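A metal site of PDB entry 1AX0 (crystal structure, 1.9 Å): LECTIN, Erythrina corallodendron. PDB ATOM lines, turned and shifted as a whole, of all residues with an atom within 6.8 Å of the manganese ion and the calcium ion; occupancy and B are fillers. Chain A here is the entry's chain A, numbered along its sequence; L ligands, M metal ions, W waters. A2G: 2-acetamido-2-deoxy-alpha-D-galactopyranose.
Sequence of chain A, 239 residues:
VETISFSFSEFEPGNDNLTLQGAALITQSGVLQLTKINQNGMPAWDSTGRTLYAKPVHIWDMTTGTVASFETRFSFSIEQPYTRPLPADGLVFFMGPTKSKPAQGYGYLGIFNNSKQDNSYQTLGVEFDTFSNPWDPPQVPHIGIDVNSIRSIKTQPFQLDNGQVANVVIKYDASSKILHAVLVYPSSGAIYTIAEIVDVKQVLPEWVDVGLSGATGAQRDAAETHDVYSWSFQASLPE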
ATOM      1  N   ASP A  89      -4.685 -25.376   4.807  1.00  0.00           N
ATOM      2  CA  ASP A  89      -5.255 -24.894   6.067  1.00  0.00           C
ATOM      3  C   ASP A  89      -6.659 -25.460   6.317  1.00  0.00           C
ATOM      4  O   ASP A  89      -7.110 -25.534   7.464  1.00  0.00           O
ATOM      5  CB  ASP A  89      -5.349 -23.367   6.064  1.00  0.00           C
ATOM      6  CG  ASP A  89      -4.124 -22.701   6.646  1.00  0.00           C
ATOM      7  OD1 ASP A  89      -3.964 -22.713   7.889  1.00  0.00           O
ATOM      8  OD2 ASP A  89      -3.309 -22.181   5.855  1.00  0.00           O
ATOM      9  N   TYR A 106      -5.003 -18.543   4.085  1.00  0.00           N
ATOM     10  CA  TYR A 106      -4.327 -19.275   5.166  1.00  0.00           C
ATOM     11  C   TYR A 106      -5.322 -19.705   6.244  1.00  0.00           C
ATOM     12  O   TYR A 106      -6.421 -20.187   5.920  1.00  0.00           O
ATOM     13  CB  TYR A 106      -3.205 -18.422   5.779  1.00  0.00           C
ATOM     14  CG  TYR A 106      -2.320 -17.753   4.749  1.00  0.00           C
ATOM     15  CD1 TYR A 106      -1.861 -18.449   3.631  1.00  0.00           C
ATOM     16  CD2 TYR A 106      -1.964 -16.416   4.881  1.00  0.00           C
ATOM     17  CE1 TYR A 106      -1.076 -17.828   2.667  1.00  0.00           C
ATOM     18  CE2 TYR A 106      -1.174 -15.782   3.920  1.00  0.00           C
ATOM     19  CZ  TYR A 106      -0.742 -16.488   2.814  1.00  0.00           C
ATOM     20  OH  TYR A 106       0.023 -15.872   1.860  1.00  0.00           O
ATOM     21  N   GLY A 107      -4.965 -19.510   7.507  1.00  0.00           N
ATOM     22  CA  GLY A 107      -5.829 -19.899   8.613  1.00  0.00           C
ATOM     23  C   GLY A 107      -7.184 -19.213   8.657  1.00  0.00           C
ATOM     24  O   GLY A 107      -8.067 -19.661   9.386  1.00  0.00           O
ATOM     25  N   TYR A 108      -7.344 -18.131   7.905  1.00  0.00           N
ATOM     26  CA  TYR A 108      -8.612 -17.402   7.864  1.00  0.00           C
ATOM     27  C   TYR A 108      -9.585 -18.023   6.876  1.00  0.00           C
ATOM     28  O   TYR A 108     -10.734 -17.592   6.764  1.00  0.00           O
ATOM     29  CB  TYR A 108      -8.380 -15.924   7.580  1.00  0.00           C
ATOM     30  CG  TYR A 108      -7.465 -15.295   8.608  1.00  0.00           C
ATOM     31  CD1 TYR A 108      -7.864 -15.183   9.932  1.00  0.00           C
ATOM     32  CD2 TYR A 108      -6.192 -14.863   8.256  1.00  0.00           C
ATOM     33  CE1 TYR A 108      -7.011 -14.668  10.890  1.00  0.00           C
ATOM     34  CE2 TYR A 108      -5.323 -14.336   9.210  1.00  0.00           C
ATOM     35  CZ  TYR A 108      -5.735 -14.243  10.532  1.00  0.00           C
ATOM     36  OH  TYR A 108      -4.895 -13.730  11.485  1.00  0.00           O
ATOM     37  N   LEU A 109      -9.090 -19.015   6.139  1.00  0.00           N
ATOM     38  CA  LEU A 109      -9.870 -19.791   5.170  1.00  0.00           C
ATOM     39  C   LEU A 109     -10.602 -19.046   4.054  1.00  0.00           C
ATOM     40  O   LEU A 109     -11.516 -19.596   3.438  1.00  0.00           O
ATOM     41  CB  LEU A 109     -10.859 -20.673   5.938  1.00  0.00           C
ATOM     42  CG  LEU A 109     -10.249 -21.548   7.052  1.00  0.00           C
ATOM     43  CD1 LEU A 109     -11.354 -22.247   7.831  1.00  0.00           C
ATOM     44  CD2 LEU A 109      -9.276 -22.554   6.456  1.00  0.00           C
ATOM     45  N   GLU A 127     -16.438 -25.159   9.419  1.00  0.00           N
ATOM     46  CA  GLU A 127     -15.113 -25.450   8.912  1.00  0.00           C
ATOM     47  C   GLU A 127     -14.611 -26.855   9.169  1.00  0.00           C
ATOM     48  O   GLU A 127     -15.047 -27.540  10.087  1.00  0.00           O
ATOM     49  CB  GLU A 127     -14.122 -24.479   9.538  1.00  0.00           C
ATOM     50  CG  GLU A 127     -14.131 -24.594  11.054  1.00  0.00           C
ATOM     51  CD  GLU A 127     -12.987 -23.897  11.702  1.00  0.00           C
ATOM     52  OE1 GLU A 127     -12.775 -22.705  11.465  1.00  0.00           O
ATOM     53  OE2 GLU A 127     -12.296 -24.588  12.473  1.00  0.00           O
ATOM     54  N   ASP A 129     -11.038 -27.779   9.522  1.00  0.00           N
ATOM     55  CA  ASP A 129      -9.726 -27.202   9.760  1.00  0.00           C
ATOM     56  C   ASP A 129      -8.600 -28.222   9.948  1.00  0.00           C
ATOM     57  O   ASP A 129      -8.637 -29.024  10.864  1.00  0.00           O
ATOM     58  CB  ASP A 129      -9.848 -26.336  10.996  1.00  0.00           C
ATOM     59  CG  ASP A 129      -8.732 -25.349  11.140  1.00  0.00           C
ATOM     60  OD1 ASP A 129      -7.650 -25.527  10.548  1.00  0.00           O
ATOM     61  OD2 ASP A 129      -8.953 -24.375  11.863  1.00  0.00           O
ATOM     62  N   THR A 130      -7.547 -28.070   9.143  1.00  0.00           N
ATOM     63  CA  THR A 130      -6.422 -28.993   9.162  1.00  0.00           C
ATOM     64  C   THR A 130      -5.127 -28.487   9.811  1.00  0.00           C
ATOM     65  O   THR A 130      -4.168 -29.254   9.962  1.00  0.00           O
ATOM     66  CB  THR A 130      -6.106 -29.464   7.734  1.00  0.00           C
ATOM     67  OG1 THR A 130      -5.835 -28.325   6.906  1.00  0.00           O
ATOM     68  CG2 THR A 130      -7.279 -30.234   7.157  1.00  0.00           C
ATOM     69  N   PHE A 131      -5.089 -27.224  10.209  1.00  0.00           N
ATOM     70  CA  PHE A 131      -3.888 -26.669  10.826  1.00  0.00           C
ATOM     71  C   PHE A 131      -4.236 -25.939  12.123  1.00  0.00           C
ATOM     72  O   PHE A 131      -5.144 -25.131  12.140  1.00  0.00           O
ATOM     73  CB  PHE A 131      -3.186 -25.708   9.855  1.00  0.00           C
ATOM     74  CG  PHE A 131      -1.923 -25.108  10.405  1.00  0.00           C
ATOM     75  CD1 PHE A 131      -0.706 -25.744  10.216  1.00  0.00           C
ATOM     76  CD2 PHE A 131      -1.955 -23.909  11.123  1.00  0.00           C
ATOM     77  CE1 PHE A 131       0.470 -25.203  10.752  1.00  0.00           C
ATOM     78  CE2 PHE A 131      -0.795 -23.363  11.659  1.00  0.00           C
ATOM     79  CZ  PHE A 131       0.430 -24.010  11.472  1.00  0.00           C
ATOM     80  N   SER A 132      -3.475 -26.205  13.181  1.00  0.00           N
ATOM     81  CA  SER A 132      -3.750 -25.564  14.463  1.00  0.00           C
ATOM     82  C   SER A 132      -3.095 -24.191  14.631  1.00  0.00           C
ATOM     83  O   SER A 132      -1.889 -24.102  14.855  1.00  0.00           O
ATOM     84  CB  SER A 132      -3.327 -26.496  15.615  1.00  0.00           C
ATOM     85  OG  SER A 132      -3.793 -25.990  16.859  1.00  0.00           O
ATOM     86  N   ASN A 133      -3.902 -23.144  14.487  1.00  0.00           N
ATOM     87  CA  ASN A 133      -3.444 -21.759  14.655  1.00  0.00           C
ATOM     88  C   ASN A 133      -3.506 -21.423  16.150  1.00  0.00           C
ATOM     89  O   ASN A 133      -4.010 -22.218  16.940  1.00  0.00           O
ATOM     90  CB  ASN A 133      -4.334 -20.805  13.848  1.00  0.00           C
ATOM     91  CG  ASN A 133      -4.244 -21.036  12.362  1.00  0.00           C
ATOM     92  OD1 ASN A 133      -5.061 -21.739  11.788  1.00  0.00           O
ATOM     93  ND2 ASN A 133      -3.247 -20.434  11.718  1.00  0.00           N
ATOM     94  N   TRP A 135      -5.478 -19.620  17.767  1.00  0.00           N
ATOM     95  CA  TRP A 135      -6.870 -19.532  18.226  1.00  0.00           C
ATOM     96  C   TRP A 135      -7.591 -20.874  18.181  1.00  0.00           C
ATOM     97  O   TRP A 135      -8.763 -20.979  18.570  1.00  0.00           O
ATOM     98  CB  TRP A 135      -7.639 -18.523  17.358  1.00  0.00           C
ATOM     99  CG  TRP A 135      -7.597 -18.843  15.883  1.00  0.00           C
ATOM    100  CD1 TRP A 135      -8.320 -19.810  15.231  1.00  0.00           C
ATOM    101  CD2 TRP A 135      -6.803 -18.193  14.889  1.00  0.00           C
ATOM    102  NE1 TRP A 135      -8.018 -19.792  13.892  1.00  0.00           N
ATOM    103  CE2 TRP A 135      -7.086 -18.814  13.647  1.00  0.00           C
ATOM    104  CE3 TRP A 135      -5.865 -17.154  14.927  1.00  0.00           C
ATOM    105  CZ2 TRP A 135      -6.475 -18.417  12.459  1.00  0.00           C
ATOM    106  CZ3 TRP A 135      -5.255 -16.760  13.726  1.00  0.00           C
ATOM    107  CH2 TRP A 135      -5.573 -17.394  12.512  1.00  0.00           C
ATOM    108  N   ASP A 136      -6.891 -21.900  17.695  1.00  0.00           N
ATOM    109  CA  ASP A 136      -7.440 -23.250  17.563  1.00  0.00           C
ATOM    110  C   ASP A 136      -7.125 -24.195  18.699  1.00  0.00           C
ATOM    111  O   ASP A 136      -6.177 -23.971  19.462  1.00  0.00           O
ATOM    112  CB  ASP A 136      -6.841 -23.923  16.317  1.00  0.00           C
ATOM    113  CG  ASP A 136      -7.433 -23.411  15.047  1.00  0.00           C
ATOM    114  OD1 ASP A 136      -8.622 -23.088  15.059  1.00  0.00           O
ATOM    115  OD2 ASP A 136      -6.715 -23.306  14.043  1.00  0.00           O
ATOM    116  N   PRO A 137      -7.942 -25.245  18.849  1.00  0.00           N
ATOM    117  CA  PRO A 137      -7.681 -26.218  19.902  1.00  0.00           C
ATOM    118  C   PRO A 137      -6.479 -26.974  19.327  1.00  0.00           C
ATOM    119  O   PRO A 137      -6.228 -26.929  18.111  1.00  0.00           O
ATOM    120  CB  PRO A 137      -8.941 -27.075  19.901  1.00  0.00           C
ATOM    121  CG  PRO A 137      -9.435 -26.978  18.487  1.00  0.00           C
ATOM    122  CD  PRO A 137      -9.244 -25.515  18.195  1.00  0.00           C
ATOM    123  N   VAL A 140      -6.126 -31.399  15.447  1.00  0.00           N
ATOM    124  CA  VAL A 140      -6.448 -31.186  14.048  1.00  0.00           C
ATOM    125  C   VAL A 140      -6.351 -32.541  13.339  1.00  0.00           C
ATOM    126  O   VAL A 140      -5.542 -33.386  13.712  1.00  0.00           O
ATOM    127  CB  VAL A 140      -5.526 -30.158  13.331  1.00  0.00           C
ATOM    128  CG1 VAL A 140      -5.863 -28.744  13.772  1.00  0.00           C
ATOM    129  CG2 VAL A 140      -4.052 -30.475  13.605  1.00  0.00           C
ATOM    130  N   HIS A 142     -10.254 -30.737  12.712  1.00  0.00           N
ATOM    131  CA  HIS A 142     -11.453 -30.615  13.517  1.00  0.00           C
ATOM    132  C   HIS A 142     -12.545 -29.887  12.761  1.00  0.00           C
ATOM    133  O   HIS A 142     -12.275 -29.135  11.827  1.00  0.00           O
ATOM    134  CB  HIS A 142     -11.169 -29.923  14.859  1.00  0.00           C
ATOM    135  CG  HIS A 142     -10.563 -28.555  14.734  1.00  0.00           C
ATOM    136  ND1 HIS A 142      -9.228 -28.290  14.926  1.00  0.00           N
ATOM    137  CD2 HIS A 142     -11.138 -27.366  14.425  1.00  0.00           C
ATOM    138  CE1 HIS A 142      -9.042 -26.977  14.729  1.00  0.00           C
ATOM    139  NE2 HIS A 142     -10.174 -26.377  14.422  1.00  0.00           N
ATOM    140  N   ILE A 143     -13.778 -30.216  13.114  1.00  0.00           N
ATOM    141  CA  ILE A 143     -14.938 -29.557  12.533  1.00  0.00           C
ATOM    142  C   ILE A 143     -15.172 -28.409  13.494  1.00  0.00           C
ATOM    143  O   ILE A 143     -14.976 -28.553  14.699  1.00  0.00           O
ATOM    144  CB  ILE A 143     -16.197 -30.451  12.578  1.00  0.00           C
ATOM    145  CG1 ILE A 143     -15.921 -31.798  11.901  1.00  0.00           C
ATOM    146  CG2 ILE A 143     -17.364 -29.734  11.889  1.00  0.00           C
ATOM    147  CD1 ILE A 143     -17.063 -32.784  12.044  1.00  0.00           C
ATOM    148  N   GLY A 144     -15.585 -27.258  12.974  1.00  0.00           N
ATOM    149  CA  GLY A 144     -15.843 -26.141  13.857  1.00  0.00           C
ATOM    150  C   GLY A 144     -16.996 -25.300  13.364  1.00  0.00           C
ATOM    151  O   GLY A 144     -17.223 -25.196  12.171  1.00  0.00           O
ATOM    152  N   ASP A 146     -18.300 -21.659  13.176  1.00  0.00           N
ATOM    153  CA  ASP A 146     -17.798 -20.283  13.249  1.00  0.00           C
ATOM    154  C   ASP A 146     -18.914 -19.251  13.137  1.00  0.00           C
ATOM    155  O   ASP A 146     -19.625 -19.207  12.142  1.00  0.00           O
ATOM    156  CB  ASP A 146     -16.796 -20.046  12.107  1.00  0.00           C
ATOM    157  CG  ASP A 146     -15.623 -21.011  12.139  1.00  0.00           C
ATOM    158  OD1 ASP A 146     -15.476 -21.738  13.144  1.00  0.00           O
ATOM    159  OD2 ASP A 146     -14.847 -21.044  11.169  1.00  0.00           O
ATOM    160  N   ILE A 150     -13.237 -16.652  13.320  1.00  0.00           N
ATOM    161  CA  ILE A 150     -12.498 -17.867  12.985  1.00  0.00           C
ATOM    162  C   ILE A 150     -12.314 -18.678  14.284  1.00  0.00           C
ATOM    163  O   ILE A 150     -11.954 -19.855  14.245  1.00  0.00           O
ATOM    164  CB  ILE A 150     -11.127 -17.509  12.327  1.00  0.00           C
ATOM    165  CG1 ILE A 150     -10.480 -18.751  11.715  1.00  0.00           C
ATOM    166  CG2 ILE A 150     -10.227 -16.798  13.330  1.00  0.00           C
ATOM    167  CD1 ILE A 150     -11.259 -19.327  10.537  1.00  0.00           C
ATOM    168  N   ARG A 151     -12.544 -18.027  15.428  1.00  0.00           N
ATOM    169  CA  ARG A 151     -12.464 -18.694  16.724  1.00  0.00           C
ATOM    170  C   ARG A 151     -13.813 -19.368  16.937  1.00  0.00           C
ATOM    171  O   ARG A 151     -14.756 -18.745  17.409  1.00  0.00           O
ATOM    172  CB  ARG A 151     -12.229 -17.698  17.852  1.00  0.00           C
ATOM    173  CG  ARG A 151     -10.991 -16.828  17.706  1.00  0.00           C
ATOM    174  CD  ARG A 151     -10.697 -16.141  19.026  1.00  0.00           C
ATOM    175  NE  ARG A 151     -10.594 -14.693  18.885  1.00  0.00           N
ATOM    176  CZ  ARG A 151     -11.367 -13.822  19.531  1.00  0.00           C
ATOM    177  NH1 ARG A 151     -12.301 -14.243  20.382  1.00  0.00           N
ATOM    178  NH2 ARG A 151     -11.194 -12.527  19.332  1.00  0.00           N
ATOM    179  N   SER A 152     -13.881 -20.668  16.616  1.00  0.00           N
ATOM    180  CA  SER A 152     -15.117 -21.437  16.709  1.00  0.00           C
ATOM    181  C   SER A 152     -15.798 -21.445  18.074  1.00  0.00           C
ATOM    182  O   SER A 152     -15.136 -21.477  19.107  1.00  0.00           O
ATOM    183  CB  SER A 152     -14.871 -22.890  16.294  1.00  0.00           C
ATOM    184  OG  SER A 152     -14.194 -22.956  15.050  1.00  0.00           O
ATOM    185  N   THR A 155     -16.081 -27.031  18.637  1.00  0.00           N
ATOM    186  CA  THR A 155     -15.229 -27.819  17.752  1.00  0.00           C
ATOM    187  C   THR A 155     -15.344 -29.311  18.058  1.00  0.00           C
ATOM    188  O   THR A 155     -15.712 -29.705  19.171  1.00  0.00           O
ATOM    189  CB  THR A 155     -13.751 -27.377  17.867  1.00  0.00           C
ATOM    190  OG1 THR A 155     -12.970 -28.043  16.858  1.00  0.00           O
ATOM    191  CG2 THR A 155     -13.186 -27.735  19.220  1.00  0.00           C
HETATM  192  O5  A2G L   1       1.502 -20.655   8.227  1.00  0.00           O
HETATM  193  C1  A2G L   1       1.030 -19.652   9.135  1.00  0.00           C
HETATM  194  O1  A2G L   1       1.331 -20.071  10.417  1.00  0.00           O
HETATM  195  C2  A2G L   1      -0.486 -19.471   8.999  1.00  0.00           C
HETATM  196  N2  A2G L   1      -0.953 -18.552  10.029  1.00  0.00           N
HETATM  197  C3  A2G L   1      -1.222 -20.809   9.145  1.00  0.00           C
HETATM  198  O3  A2G L   1      -2.608 -20.631   8.874  1.00  0.00           O
HETATM  199  C4  A2G L   1      -0.624 -21.831   8.186  1.00  0.00           C
HETATM  200  O4  A2G L   1      -0.853 -21.411   6.845  1.00  0.00           O
HETATM  201  C5  A2G L   1       0.875 -21.943   8.445  1.00  0.00           C
HETATM  202  C6  A2G L   1       1.558 -22.928   7.528  1.00  0.00           C
HETATM  203  O6  A2G L   1       2.876 -23.212   7.968  1.00  0.00           O
HETATM  204  C7  A2G L   1      -1.627 -17.462   9.695  1.00  0.00           C
HETATM  205  O7  A2G L   1      -1.898 -17.160   8.539  1.00  0.00           O
HETATM  206  C8  A2G L   1      -2.078 -16.558  10.836  1.00  0.00           C
HETATM  207 MN    MN M   1     -10.352 -24.057  13.742  1.00  0.00          MN
HETATM  208 CA    CA M   2      -6.741 -23.439  11.625  1.00  0.00          CA
HETATM  209  O   HOH W   1      -8.269 -21.564  11.300  1.00  0.00           O
HETATM  210  O   HOH W   2     -11.728 -23.730  15.726  1.00  0.00           O
HETATM  211  O   HOH W   3      -6.148 -23.431   9.262  1.00  0.00           O
HETATM  212  O   HOH W   4     -10.709 -21.775  12.898  1.00  0.00           O
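ND2 of Asn 133 lies within hydrogen-bond range of O3 of the ligand (2.9 Å).
O3 of the ligand sits at hydrogen-bond distance from N of Gly 107 (2.9 Å).
OD1 of Asp 89 lies within hydrogen-bond range of O3 of the ligand.
OE1 of Glu 127 lies close to OD2 of Asp 146.
N of Glu 127 lies within hydrogen-bond range of O of Gly 144 (2.9 Å).
Within 4 Å of the manganese ion: Glu 127, Asp 129, Asp 136 and His 142.
The nearest printed residue that does not touch the manganese ion is Ser 152 (4.2 Å).
Within 4 Å of the calcium ion: Asp 129, Phe 131, Asn 133 and Asp 136.
The nearest printed residue that does not touch the calcium ion is Trp 135 (4.5 Å).
The side-chain carboxylate (OD2) of Asp 129 binds the manganese ion (2.4 Å).
The manganese ion is bound by OD1 of Asp 136 (2.4 Å).
OE2 of Glu 127 is bound to the manganese ion (2.4 Å).
NE2 of His 142 is bound to the manganese ion (2.4 Å).
Water W2 is bound to the manganese ion (2.4 Å).
The manganese ion is bound by water W4, at 2.5 Å.
The calcium ion is bound by O of Phe 131 (2.4 Å), OD1 of Asn 133 (2.4 Å), OD2 of Asp 129 (2.4 Å), OD2 of Asp 136 (2.4 Å), water W3 (2.4 Å), water W1 (2.4 Å) and OD1 of Asp 129 (2.5 Å).
Water W4 lies within hydrogen-bond range of O of Ile 150 (2.7 Å), OE1 of Glu 127 (2.7 Å) and NE1 of Trp 135 (3.5 Å).
Water W1 bridges the backbone carbonyl oxygen (O) of Gly 107 (2.7 Å) and the indole nitrogen (NE1) of Trp 135 (3.1 Å).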
